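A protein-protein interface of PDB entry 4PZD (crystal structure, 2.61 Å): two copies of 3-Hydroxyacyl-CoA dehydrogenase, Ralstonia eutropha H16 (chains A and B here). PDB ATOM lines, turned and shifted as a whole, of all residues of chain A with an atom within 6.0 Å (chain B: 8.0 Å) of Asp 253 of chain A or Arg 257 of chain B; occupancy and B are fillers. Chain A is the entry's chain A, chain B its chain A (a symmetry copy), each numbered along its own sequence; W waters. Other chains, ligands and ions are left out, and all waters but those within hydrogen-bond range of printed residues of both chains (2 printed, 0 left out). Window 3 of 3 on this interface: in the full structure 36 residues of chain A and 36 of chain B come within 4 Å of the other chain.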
ATOM      1  N   LEU A 247     -23.653  27.001  40.332  1.00  0.00           N
ATOM      2  CA  LEU A 247     -23.176  27.246  39.002  1.00  0.00           C
ATOM      3  C   LEU A 247     -24.234  26.816  37.986  1.00  0.00           C
ATOM      4  O   LEU A 247     -24.604  27.591  37.091  1.00  0.00           O
ATOM      5  CB  LEU A 247     -21.883  26.500  38.787  1.00  0.00           C
ATOM      6  CG  LEU A 247     -20.662  27.087  39.513  1.00  0.00           C
ATOM      7  CD1 LEU A 247     -19.373  26.420  39.051  1.00  0.00           C
ATOM      8  CD2 LEU A 247     -20.534  28.574  39.280  1.00  0.00           C
ATOM      9  N   TYR A 248     -24.763  25.603  38.144  1.00  0.00           N
ATOM     10  CA  TYR A 248     -25.766  25.076  37.191  1.00  0.00           C
ATOM     11  C   TYR A 248     -27.083  25.865  37.192  1.00  0.00           C
ATOM     12  O   TYR A 248     -27.743  26.003  36.174  1.00  0.00           O
ATOM     13  CB  TYR A 248     -25.992  23.574  37.424  1.00  0.00           C
ATOM     14  CG  TYR A 248     -27.163  23.012  36.686  1.00  0.00           C
ATOM     15  CD1 TYR A 248     -27.219  23.096  35.313  1.00  0.00           C
ATOM     16  CD2 TYR A 248     -28.249  22.424  37.365  1.00  0.00           C
ATOM     17  CE1 TYR A 248     -28.302  22.622  34.603  1.00  0.00           C
ATOM     18  CE2 TYR A 248     -29.348  21.932  36.663  1.00  0.00           C
ATOM     19  CZ  TYR A 248     -29.364  22.035  35.281  1.00  0.00           C
ATOM     20  OH  TYR A 248     -30.396  21.574  34.545  1.00  0.00           O
ATOM     21  N   THR A 249     -27.433  26.441  38.324  1.00  0.00           N
ATOM     22  CA  THR A 249     -28.717  27.061  38.480  1.00  0.00           C
ATOM     23  C   THR A 249     -28.601  28.473  38.049  1.00  0.00           C
ATOM     24  O   THR A 249     -29.412  28.966  37.294  1.00  0.00           O
ATOM     25  CB  THR A 249     -29.205  26.918  39.937  1.00  0.00           C
ATOM     26  OG1 THR A 249     -29.519  25.540  40.157  1.00  0.00           O
ATOM     27  CG2 THR A 249     -30.468  27.709  40.181  1.00  0.00           C
ATOM     28  N   PHE A 251     -26.251  29.892  36.078  1.00  0.00           N
ATOM     29  CA  PHE A 251     -25.976  29.972  34.606  1.00  0.00           C
ATOM     30  C   PHE A 251     -27.049  29.327  33.747  1.00  0.00           C
ATOM     31  O   PHE A 251     -27.136  29.639  32.538  1.00  0.00           O
ATOM     32  CB  PHE A 251     -24.635  29.326  34.237  1.00  0.00           C
ATOM     33  CG  PHE A 251     -23.466  30.164  34.579  1.00  0.00           C
ATOM     34  CD1 PHE A 251     -23.308  31.401  34.013  1.00  0.00           C
ATOM     35  CD2 PHE A 251     -22.509  29.723  35.467  1.00  0.00           C
ATOM     36  CE1 PHE A 251     -22.214  32.209  34.332  1.00  0.00           C
ATOM     37  CE2 PHE A 251     -21.403  30.502  35.779  1.00  0.00           C
ATOM     38  CZ  PHE A 251     -21.269  31.765  35.221  1.00  0.00           C
ATOM     39  N   ALA A 252     -27.825  28.413  34.363  1.00  0.00           N
ATOM     40  CA  ALA A 252     -28.836  27.612  33.677  1.00  0.00           C
ATOM     41  C   ALA A 252     -28.233  26.908  32.487  1.00  0.00           C
ATOM     42  O   ALA A 252     -28.752  27.045  31.361  1.00  0.00           O
ATOM     43  CB  ALA A 252     -30.017  28.473  33.227  1.00  0.00           C
ATOM     44  N   ASP A 253     -27.145  26.174  32.747  1.00  0.00           N
ATOM     45  CA  ASP A 253     -26.284  25.540  31.717  1.00  0.00           C
ATOM     46  C   ASP A 253     -25.690  24.221  32.285  1.00  0.00           C
ATOM     47  O   ASP A 253     -24.905  24.241  33.263  1.00  0.00           O
ATOM     48  CB  ASP A 253     -25.158  26.522  31.286  1.00  0.00           C
ATOM     49  CG  ASP A 253     -24.278  26.013  30.116  1.00  0.00           C
ATOM     50  OD1 ASP A 253     -24.318  24.842  29.597  1.00  0.00           O
ATOM     51  OD2 ASP A 253     -23.481  26.882  29.682  1.00  0.00           O
ATOM     52  N   PRO A 254     -26.065  23.087  31.674  1.00  0.00           N
ATOM     53  CA  PRO A 254     -25.587  21.766  32.066  1.00  0.00           C
ATOM     54  C   PRO A 254     -24.099  21.550  31.954  1.00  0.00           C
ATOM     55  O   PRO A 254     -23.583  20.516  32.418  1.00  0.00           O
ATOM     56  CB  PRO A 254     -26.303  20.819  31.090  1.00  0.00           C
ATOM     57  CG  PRO A 254     -26.608  21.660  29.925  1.00  0.00           C
ATOM     58  CD  PRO A 254     -27.002  22.980  30.542  1.00  0.00           C
ATOM     59  N   LYS A 255     -23.400  22.478  31.325  1.00  0.00           N
ATOM     60  CA  LYS A 255     -21.946  22.416  31.326  1.00  0.00           C
ATOM     61  C   LYS A 255     -21.445  22.169  32.775  1.00  0.00           C
ATOM     62  O   LYS A 255     -20.502  21.430  32.996  1.00  0.00           O
ATOM     63  CB  LYS A 255     -21.372  23.705  30.761  1.00  0.00           C
ATOM     64  CG  LYS A 255     -19.902  23.815  31.069  1.00  0.00           C
ATOM     65  CD  LYS A 255     -19.213  24.910  30.301  1.00  0.00           C
ATOM     66  CE  LYS A 255     -17.755  24.911  30.745  1.00  0.00           C
ATOM     67  NZ  LYS A 255     -17.071  26.209  30.546  1.00  0.00           N
ATOM     68  N   TYR A 256     -22.130  22.775  33.748  1.00  0.00           N
ATOM     69  CA  TYR A 256     -21.850  22.608  35.178  1.00  0.00           C
ATOM     70  C   TYR A 256     -22.717  21.543  35.904  1.00  0.00           C
ATOM     71  O   TYR A 256     -22.946  21.669  37.076  1.00  0.00           O
ATOM     72  CB  TYR A 256     -22.008  23.981  35.859  1.00  0.00           C
ATOM     73  CG  TYR A 256     -21.247  25.090  35.106  1.00  0.00           C
ATOM     74  CD1 TYR A 256     -19.922  25.350  35.409  1.00  0.00           C
ATOM     75  CD2 TYR A 256     -21.850  25.842  34.082  1.00  0.00           C
ATOM     76  CE1 TYR A 256     -19.205  26.324  34.737  1.00  0.00           C
ATOM     77  CE2 TYR A 256     -21.153  26.821  33.399  1.00  0.00           C
ATOM     78  CZ  TYR A 256     -19.808  27.052  33.741  1.00  0.00           C
ATOM     79  OH  TYR A 256     -19.020  27.960  33.099  1.00  0.00           O
ATOM     80  N   ARG A 257     -23.229  20.520  35.210  1.00  0.00           N
ATOM     81  CA  ARG A 257     -23.853  19.358  35.875  1.00  0.00           C
ATOM     82  C   ARG A 257     -23.024  18.979  37.066  1.00  0.00           C
ATOM     83  O   ARG A 257     -21.834  18.706  36.917  1.00  0.00           O
ATOM     84  CB  ARG A 257     -23.711  18.112  34.992  1.00  0.00           C
ATOM     85  CG  ARG A 257     -24.873  17.727  34.125  1.00  0.00           C
ATOM     86  CD  ARG A 257     -24.373  16.702  33.082  1.00  0.00           C
ATOM     87  NE  ARG A 257     -23.711  17.441  32.028  1.00  0.00           N
ATOM     88  CZ  ARG A 257     -23.161  16.934  30.945  1.00  0.00           C
ATOM     89  NH1 ARG A 257     -23.159  15.643  30.745  1.00  0.00           N
ATOM     90  NH2 ARG A 257     -22.606  17.750  30.055  1.00  0.00           N
ATOM     91  N   PRO B 195      -9.644  21.485  31.020  1.00  0.00           N
ATOM     92  CA  PRO B 195     -10.906  22.275  31.100  1.00  0.00           C
ATOM     93  C   PRO B 195     -10.888  23.367  32.181  1.00  0.00           C
ATOM     94  O   PRO B 195     -11.662  24.314  32.135  1.00  0.00           O
ATOM     95  CB  PRO B 195     -11.987  21.210  31.340  1.00  0.00           C
ATOM     96  CG  PRO B 195     -11.413  19.978  30.701  1.00  0.00           C
ATOM     97  CD  PRO B 195      -9.914  20.039  30.931  1.00  0.00           C
ATOM     98  N   ASN B 198      -9.282  26.191  30.357  1.00  0.00           N
ATOM     99  CA  ASN B 198     -10.407  26.679  29.560  1.00  0.00           C
ATOM    100  C   ASN B 198     -11.394  27.558  30.325  1.00  0.00           C
ATOM    101  O   ASN B 198     -11.861  28.574  29.816  1.00  0.00           O
ATOM    102  CB  ASN B 198     -11.171  25.510  28.943  1.00  0.00           C
ATOM    103  CG  ASN B 198     -11.933  25.912  27.704  1.00  0.00           C
ATOM    104  OD1 ASN B 198     -13.107  25.674  27.590  1.00  0.00           O
ATOM    105  ND2 ASN B 198     -11.243  26.505  26.762  1.00  0.00           N
ATOM    106  N   GLU B 199     -11.709  27.187  31.561  1.00  0.00           N
ATOM    107  CA  GLU B 199     -12.594  28.024  32.354  1.00  0.00           C
ATOM    108  C   GLU B 199     -11.993  29.367  32.693  1.00  0.00           C
ATOM    109  O   GLU B 199     -12.744  30.318  32.810  1.00  0.00           O
ATOM    110  CB  GLU B 199     -12.999  27.333  33.657  1.00  0.00           C
ATOM    111  CG  GLU B 199     -14.359  27.802  34.190  1.00  0.00           C
ATOM    112  CD  GLU B 199     -15.502  27.505  33.217  1.00  0.00           C
ATOM    113  OE1 GLU B 199     -15.277  26.719  32.269  1.00  0.00           O
ATOM    114  OE2 GLU B 199     -16.627  28.042  33.409  1.00  0.00           O
ATOM    115  N   CYS B 202     -12.620  31.416  29.858  1.00  0.00           N
ATOM    116  CA  CYS B 202     -14.013  31.824  29.887  1.00  0.00           C
ATOM    117  C   CYS B 202     -14.202  33.039  30.832  1.00  0.00           C
ATOM    118  O   CYS B 202     -14.915  34.004  30.505  1.00  0.00           O
ATOM    119  CB  CYS B 202     -14.942  30.635  30.234  1.00  0.00           C
ATOM    120  SG  CYS B 202     -15.229  29.396  28.911  1.00  0.00           S
ATOM    121  N   LEU B 241      -6.098  24.593  22.751  1.00  0.00           N
ATOM    122  CA  LEU B 241      -7.285  24.574  21.904  1.00  0.00           C
ATOM    123  C   LEU B 241      -7.522  23.192  21.319  1.00  0.00           C
ATOM    124  O   LEU B 241      -8.628  22.679  21.287  1.00  0.00           O
ATOM    125  CB  LEU B 241      -7.108  25.582  20.786  1.00  0.00           C
ATOM    126  CG  LEU B 241      -8.197  25.650  19.743  1.00  0.00           C
ATOM    127  CD1 LEU B 241      -9.525  25.881  20.423  1.00  0.00           C
ATOM    128  CD2 LEU B 241      -7.890  26.791  18.777  1.00  0.00           C
ATOM    129  N   MET B 244      -8.882  20.780  23.974  1.00  0.00           N
ATOM    130  CA  MET B 244     -10.313  21.036  24.118  1.00  0.00           C
ATOM    131  C   MET B 244     -11.096  20.587  22.906  1.00  0.00           C
ATOM    132  O   MET B 244     -12.150  20.070  23.028  1.00  0.00           O
ATOM    133  CB  MET B 244     -10.586  22.520  24.412  1.00  0.00           C
ATOM    134  CG  MET B 244     -10.046  23.036  25.757  1.00  0.00           C
ATOM    135  SD  MET B 244     -10.700  22.202  27.231  1.00  0.00           S
ATOM    136  CE  MET B 244      -9.452  20.965  27.284  1.00  0.00           C
ATOM    137  N   GLU B 245     -10.575  20.769  21.714  1.00  0.00           N
ATOM    138  CA  GLU B 245     -11.318  20.348  20.547  1.00  0.00           C
ATOM    139  C   GLU B 245     -11.462  18.841  20.573  1.00  0.00           C
ATOM    140  O   GLU B 245     -12.465  18.310  20.112  1.00  0.00           O
ATOM    141  CB  GLU B 245     -10.615  20.787  19.271  1.00  0.00           C
ATOM    142  CG  GLU B 245     -10.531  22.297  19.132  1.00  0.00           C
ATOM    143  CD  GLU B 245     -11.389  22.880  18.033  1.00  0.00           C
ATOM    144  OE1 GLU B 245     -12.623  22.658  18.052  1.00  0.00           O
ATOM    145  OE2 GLU B 245     -10.817  23.581  17.158  1.00  0.00           O
ATOM    146  N   LEU B 247     -11.519  16.891  23.365  1.00  0.00           N
ATOM    147  CA  LEU B 247     -12.511  16.595  24.358  1.00  0.00           C
ATOM    148  C   LEU B 247     -13.908  16.780  23.764  1.00  0.00           C
ATOM    149  O   LEU B 247     -14.759  15.884  23.857  1.00  0.00           O
ATOM    150  CB  LEU B 247     -12.307  17.490  25.554  1.00  0.00           C
ATOM    151  CG  LEU B 247     -11.090  17.145  26.426  1.00  0.00           C
ATOM    152  CD1 LEU B 247     -11.102  17.940  27.726  1.00  0.00           C
ATOM    153  CD2 LEU B 247     -11.046  15.675  26.772  1.00  0.00           C
ATOM    154  N   TYR B 248     -14.137  17.918  23.108  1.00  0.00           N
ATOM    155  CA  TYR B 248     -15.468  18.212  22.530  1.00  0.00           C
ATOM    156  C   TYR B 248     -15.870  17.253  21.402  1.00  0.00           C
ATOM    157  O   TYR B 248     -17.035  16.933  21.223  1.00  0.00           O
ATOM    158  CB  TYR B 248     -15.551  19.683  22.094  1.00  0.00           C
ATOM    159  CG  TYR B 248     -16.757  20.009  21.274  1.00  0.00           C
ATOM    160  CD1 TYR B 248     -18.017  19.794  21.783  1.00  0.00           C
ATOM    161  CD2 TYR B 248     -16.642  20.500  19.958  1.00  0.00           C
ATOM    162  CE1 TYR B 248     -19.151  20.048  21.039  1.00  0.00           C
ATOM    163  CE2 TYR B 248     -17.777  20.770  19.195  1.00  0.00           C
ATOM    164  CZ  TYR B 248     -19.027  20.541  19.746  1.00  0.00           C
ATOM    165  OH  TYR B 248     -20.163  20.786  19.061  1.00  0.00           O
ATOM    166  N   THR B 249     -14.895  16.739  20.679  1.00  0.00           N
ATOM    167  CA  THR B 249     -15.167  15.964  19.504  1.00  0.00           C
ATOM    168  C   THR B 249     -15.319  14.548  19.911  1.00  0.00           C
ATOM    169  O   THR B 249     -16.254  13.881  19.521  1.00  0.00           O
ATOM    170  CB  THR B 249     -14.049  16.169  18.459  1.00  0.00           C
ATOM    171  OG1 THR B 249     -14.161  17.504  17.960  1.00  0.00           O
ATOM    172  CG2 THR B 249     -14.209  15.236  17.282  1.00  0.00           C
ATOM    173  N   ASP B 253     -19.900  16.535  23.164  1.00  0.00           N
ATOM    174  CA  ASP B 253     -20.591  17.187  24.305  1.00  0.00           C
ATOM    175  C   ASP B 253     -20.025  18.621  24.498  1.00  0.00           C
ATOM    176  O   ASP B 253     -18.826  18.799  24.820  1.00  0.00           O
ATOM    177  CB  ASP B 253     -20.410  16.335  25.593  1.00  0.00           C
ATOM    178  CG  ASP B 253     -21.204  16.853  26.820  1.00  0.00           C
ATOM    179  OD1 ASP B 253     -21.854  17.954  26.886  1.00  0.00           O
ATOM    180  OD2 ASP B 253     -21.169  16.067  27.799  1.00  0.00           O
ATOM    181  N   PRO B 254     -20.885  19.632  24.299  1.00  0.00           N
ATOM    182  CA  PRO B 254     -20.524  21.037  24.457  1.00  0.00           C
ATOM    183  C   PRO B 254     -20.078  21.445  25.838  1.00  0.00           C
ATOM    184  O   PRO B 254     -19.597  22.579  26.027  1.00  0.00           O
ATOM    185  CB  PRO B 254     -21.823  21.783  24.111  1.00  0.00           C
ATOM    186  CG  PRO B 254     -22.886  20.806  24.380  1.00  0.00           C
ATOM    187  CD  PRO B 254     -22.294  19.505  23.891  1.00  0.00           C
ATOM    188  N   LYS B 255     -20.250  20.570  26.812  1.00  0.00           N
ATOM    189  CA  LYS B 255     -19.692  20.832  28.130  1.00  0.00           C
ATOM    190  C   LYS B 255     -18.212  21.277  27.981  1.00  0.00           C
ATOM    191  O   LYS B 255     -17.746  22.156  28.683  1.00  0.00           O
ATOM    192  CB  LYS B 255     -19.805  19.589  28.998  1.00  0.00           C
ATOM    193  CG  LYS B 255     -18.938  19.712  30.222  1.00  0.00           C
ATOM    194  CD  LYS B 255     -19.219  18.658  31.258  1.00  0.00           C
ATOM    195  CE  LYS B 255     -18.247  18.898  32.408  1.00  0.00           C
ATOM    196  NZ  LYS B 255     -17.982  17.695  33.228  1.00  0.00           N
ATOM    197  N   TYR B 256     -17.508  20.673  27.020  1.00  0.00           N
ATOM    198  CA  TYR B 256     -16.120  21.006  26.684  1.00  0.00           C
ATOM    199  C   TYR B 256     -15.943  22.002  25.505  1.00  0.00           C
ATOM    200  O   TYR B 256     -14.947  21.952  24.836  1.00  0.00           O
ATOM    201  CB  TYR B 256     -15.371  19.692  26.390  1.00  0.00           C
ATOM    202  CG  TYR B 256     -15.608  18.635  27.487  1.00  0.00           C
ATOM    203  CD1 TYR B 256     -14.781  18.589  28.596  1.00  0.00           C
ATOM    204  CD2 TYR B 256     -16.671  17.716  27.418  1.00  0.00           C
ATOM    205  CE1 TYR B 256     -14.979  17.667  29.608  1.00  0.00           C
ATOM    206  CE2 TYR B 256     -16.887  16.786  28.417  1.00  0.00           C
ATOM    207  CZ  TYR B 256     -16.020  16.775  29.525  1.00  0.00           C
ATOM    208  OH  TYR B 256     -16.173  15.931  30.584  1.00  0.00           O
ATOM    209  N   ARG B 257     -16.916  22.877  25.226  1.00  0.00           N
ATOM    210  CA  ARG B 257     -16.714  23.997  24.284  1.00  0.00           C
ATOM    211  C   ARG B 257     -15.359  24.593  24.525  1.00  0.00           C
ATOM    212  O   ARG B 257     -15.069  25.014  25.644  1.00  0.00           O
ATOM    213  CB  ARG B 257     -17.634  25.165  24.656  1.00  0.00           C
ATOM    214  CG  ARG B 257     -18.930  25.306  23.911  1.00  0.00           C
ATOM    215  CD  ARG B 257     -19.827  26.291  24.694  1.00  0.00           C
ATOM    216  NE  ARG B 257     -20.428  25.558  25.789  1.00  0.00           N
ATOM    217  CZ  ARG B 257     -21.270  26.036  26.679  1.00  0.00           C
ATOM    218  NH1 ARG B 257     -21.631  27.292  26.644  1.00  0.00           N
ATOM    219  NH2 ARG B 257     -21.752  25.227  27.617  1.00  0.00           N
ATOM    220  N   PRO B 258     -14.543  24.719  23.501  1.00  0.00           N
ATOM    221  CA  PRO B 258     -13.444  25.662  23.739  1.00  0.00           C
ATOM    222  C   PRO B 258     -13.938  27.074  24.052  1.00  0.00           C
ATOM    223  O   PRO B 258     -14.897  27.523  23.449  1.00  0.00           O
ATOM    224  CB  PRO B 258     -12.681  25.667  22.413  1.00  0.00           C
ATOM    225  CG  PRO B 258     -13.053  24.401  21.757  1.00  0.00           C
ATOM    226  CD  PRO B 258     -14.302  23.836  22.360  1.00  0.00           C
ATOM    227  N   ALA B 259     -13.291  27.748  25.001  1.00  0.00           N
ATOM    228  CA  ALA B 259     -13.490  29.193  25.251  1.00  0.00           C
ATOM    229  C   ALA B 259     -13.238  30.011  23.996  1.00  0.00           C
ATOM    230  O   ALA B 259     -12.287  29.722  23.243  1.00  0.00           O
ATOM    231  CB  ALA B 259     -12.547  29.687  26.351  1.00  0.00           C
ATOM    232  N   MET B 260     -14.057  31.031  23.789  1.00  0.00           N
ATOM    233  CA  MET B 260     -14.021  31.762  22.546  1.00  0.00           C
ATOM    234  C   MET B 260     -12.751  32.616  22.420  1.00  0.00           C
ATOM    235  O   MET B 260     -12.115  32.658  21.361  1.00  0.00           O
ATOM    236  CB  MET B 260     -15.286  32.593  22.398  1.00  0.00           C
ATOM    237  CG  MET B 260     -16.512  31.743  22.079  1.00  0.00           C
ATOM    238  SD  MET B 260     -16.525  30.958  20.463  1.00  0.00           S
ATOM    239  CE  MET B 260     -16.036  29.349  20.988  1.00  0.00           C
ATOM    240  N   MET B 262      -9.996  31.883  23.603  1.00  0.00           N
ATOM    241  CA  MET B 262      -8.930  30.945  23.276  1.00  0.00           C
ATOM    242  C   MET B 262      -8.876  30.757  21.764  1.00  0.00           C
ATOM    243  O   MET B 262      -7.786  30.672  21.185  1.00  0.00           O
ATOM    244  CB  MET B 262      -9.105  29.599  24.000  1.00  0.00           C
ATOM    245  CG  MET B 262      -7.842  28.776  24.019  1.00  0.00           C
ATOM    246  SD  MET B 262      -8.142  27.081  24.545  1.00  0.00           S
ATOM    247  CE  MET B 262      -8.141  27.275  26.325  1.00  0.00           C
ATOM    248  N   ARG B 263     -10.049  30.698  21.137  1.00  0.00           N
ATOM    249  CA  ARG B 263     -10.119  30.517  19.701  1.00  0.00           C
ATOM    250  C   ARG B 263      -9.524  31.696  18.962  1.00  0.00           C
ATOM    251  O   ARG B 263      -8.909  31.510  17.925  1.00  0.00           O
ATOM    252  CB  ARG B 263     -11.545  30.373  19.228  1.00  0.00           C
ATOM    253  CG  ARG B 263     -12.106  28.984  19.325  1.00  0.00           C
ATOM    254  CD  ARG B 263     -13.448  28.931  18.585  1.00  0.00           C
ATOM    255  NE  ARG B 263     -14.313  27.848  19.022  1.00  0.00           N
ATOM    256  CZ  ARG B 263     -14.178  26.561  18.700  1.00  0.00           C
ATOM    257  NH1 ARG B 263     -13.204  26.159  17.914  1.00  0.00           N
ATOM    258  NH2 ARG B 263     -15.062  25.660  19.176  1.00  0.00           N
HETATM  259  O   HOH W   1     -16.462  24.477  27.919  1.00  0.00           O
HETATM  260  O   HOH W   2     -20.378  19.249  34.684  1.00  0.00           O
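Asp 253 of chain A touches Arg 257 of chain B, and with the chains exchanged Arg 257 of chain A touches Asp 253 of chain B.
Lys 255 of chain B touches its own counterpart, Lys 255 of chain A.
Lys 255 of chain A touches Arg 257 of chain B, and with the chains exchanged Arg 257 of chain A touches Lys 255 of chain B.
Of the 7 pairs that touch across the chains among the printed residues, 5 have their exchanged pair printed and touching as well.
Of chain B, only Arg 257 (3.2 Å) comes within 4 Å of Asp 253 of chain A.
Printed residues of chain B within 4 Å of Tyr 256 of chain A: Glu 199.
Glu 245 of chain B touches none of the printed residues of chain A.
Pro 254 of chain B touches none of the printed residues of chain A.
Printed residues of chain A within 4 Å of Lys 255 of chain B: Lys 255 and Arg 257.
Of chain A, only Asp 253 (3.2 Å) and Lys 255 (3.5 Å) come within 4 Å of Arg 257 of chain B.
The nearest printed residue of chain B that does not touch Tyr 256 of chain A is Lys 255 of chain B (5.6 Å).
Lys 255 of chain B touches Lys 255 of chain A (CE to O, 3.4 Å).
Arg 257 of chain B touches Lys 255 of chain A.
Arg 257 of chain A touches Lys 255 of chain B (NH2 to CB, 3.5 Å).
The backbone NH (N) of Asp 253 of chain A lies within hydrogen-bond range of the backbone carbonyl oxygen (O) of Tyr 248 of chain A (3.5 Å).
N of Lys 255 of chain A sits close to OD1 of Asp 253 of chain A.
The side-chain carboxylate of Asp 253 of chain B lies close to the backbone NH of Lys 255 of chain B, 3.1 Å away.
The backbone carbonyl oxygen of Pro 254 of chain A lies within hydrogen-bond range of the guanidinium group of Arg 257 of chain A, at 3.1 Å.
O of Pro 254 of chain B is in hydrogen-bond range of NE of Arg 257 of chain B.
The side-chain amide oxygen (OD1) of Asn 198 of chain B lies close to the backbone carbonyl oxygen (O) of Arg 257 of chain B, at 2.8 Å.
The guanidinium group (NH2) of Arg 257 of chain A is in salt-bridge range of the side-chain carboxylate (OD2) of Asp 253 of chain B (3.2 Å).
OD2 of Asp 253 of chain A is in salt-bridge range of NH2 of Arg 257 of chain B (3.2 Å).
OH of Tyr 256 of chain A sits at hydrogen-bond distance from OE2 of Glu 199 of chain B (2.4 Å).
The side-chain carboxylate of Glu 199 of chain B is in salt-bridge range of the side-chain amino group of Lys 255 of chain A (2.5 Å).
Printed residues of chain B that touch a printed residue of chain A: Glu 199, Asp 253, Lys 255 and Arg 257.
Along chain B the printed residues that touch a printed residue of chain A span positions 199 to 257.
Of the 10 printed residues of chain A, 4 touch a printed residue of chain B.
Hydrophobic or aromatic side chains of chain A that line the printed part of chain B: Tyr 256.
Among the printed residues, 7 pairs touch across the chains.
Water W2 lies within hydrogen-bond range of O of Arg 257 of chain A (2.7 Å), O of Lys 255 of chain A (2.8 Å) and NZ of Lys 255 of chain B (3.2 Å).
Water W1 lies within hydrogen-bond range of O of Arg 257 of chain B, O of Lys 255 of chain B and NZ of Lys 255 of chain A.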
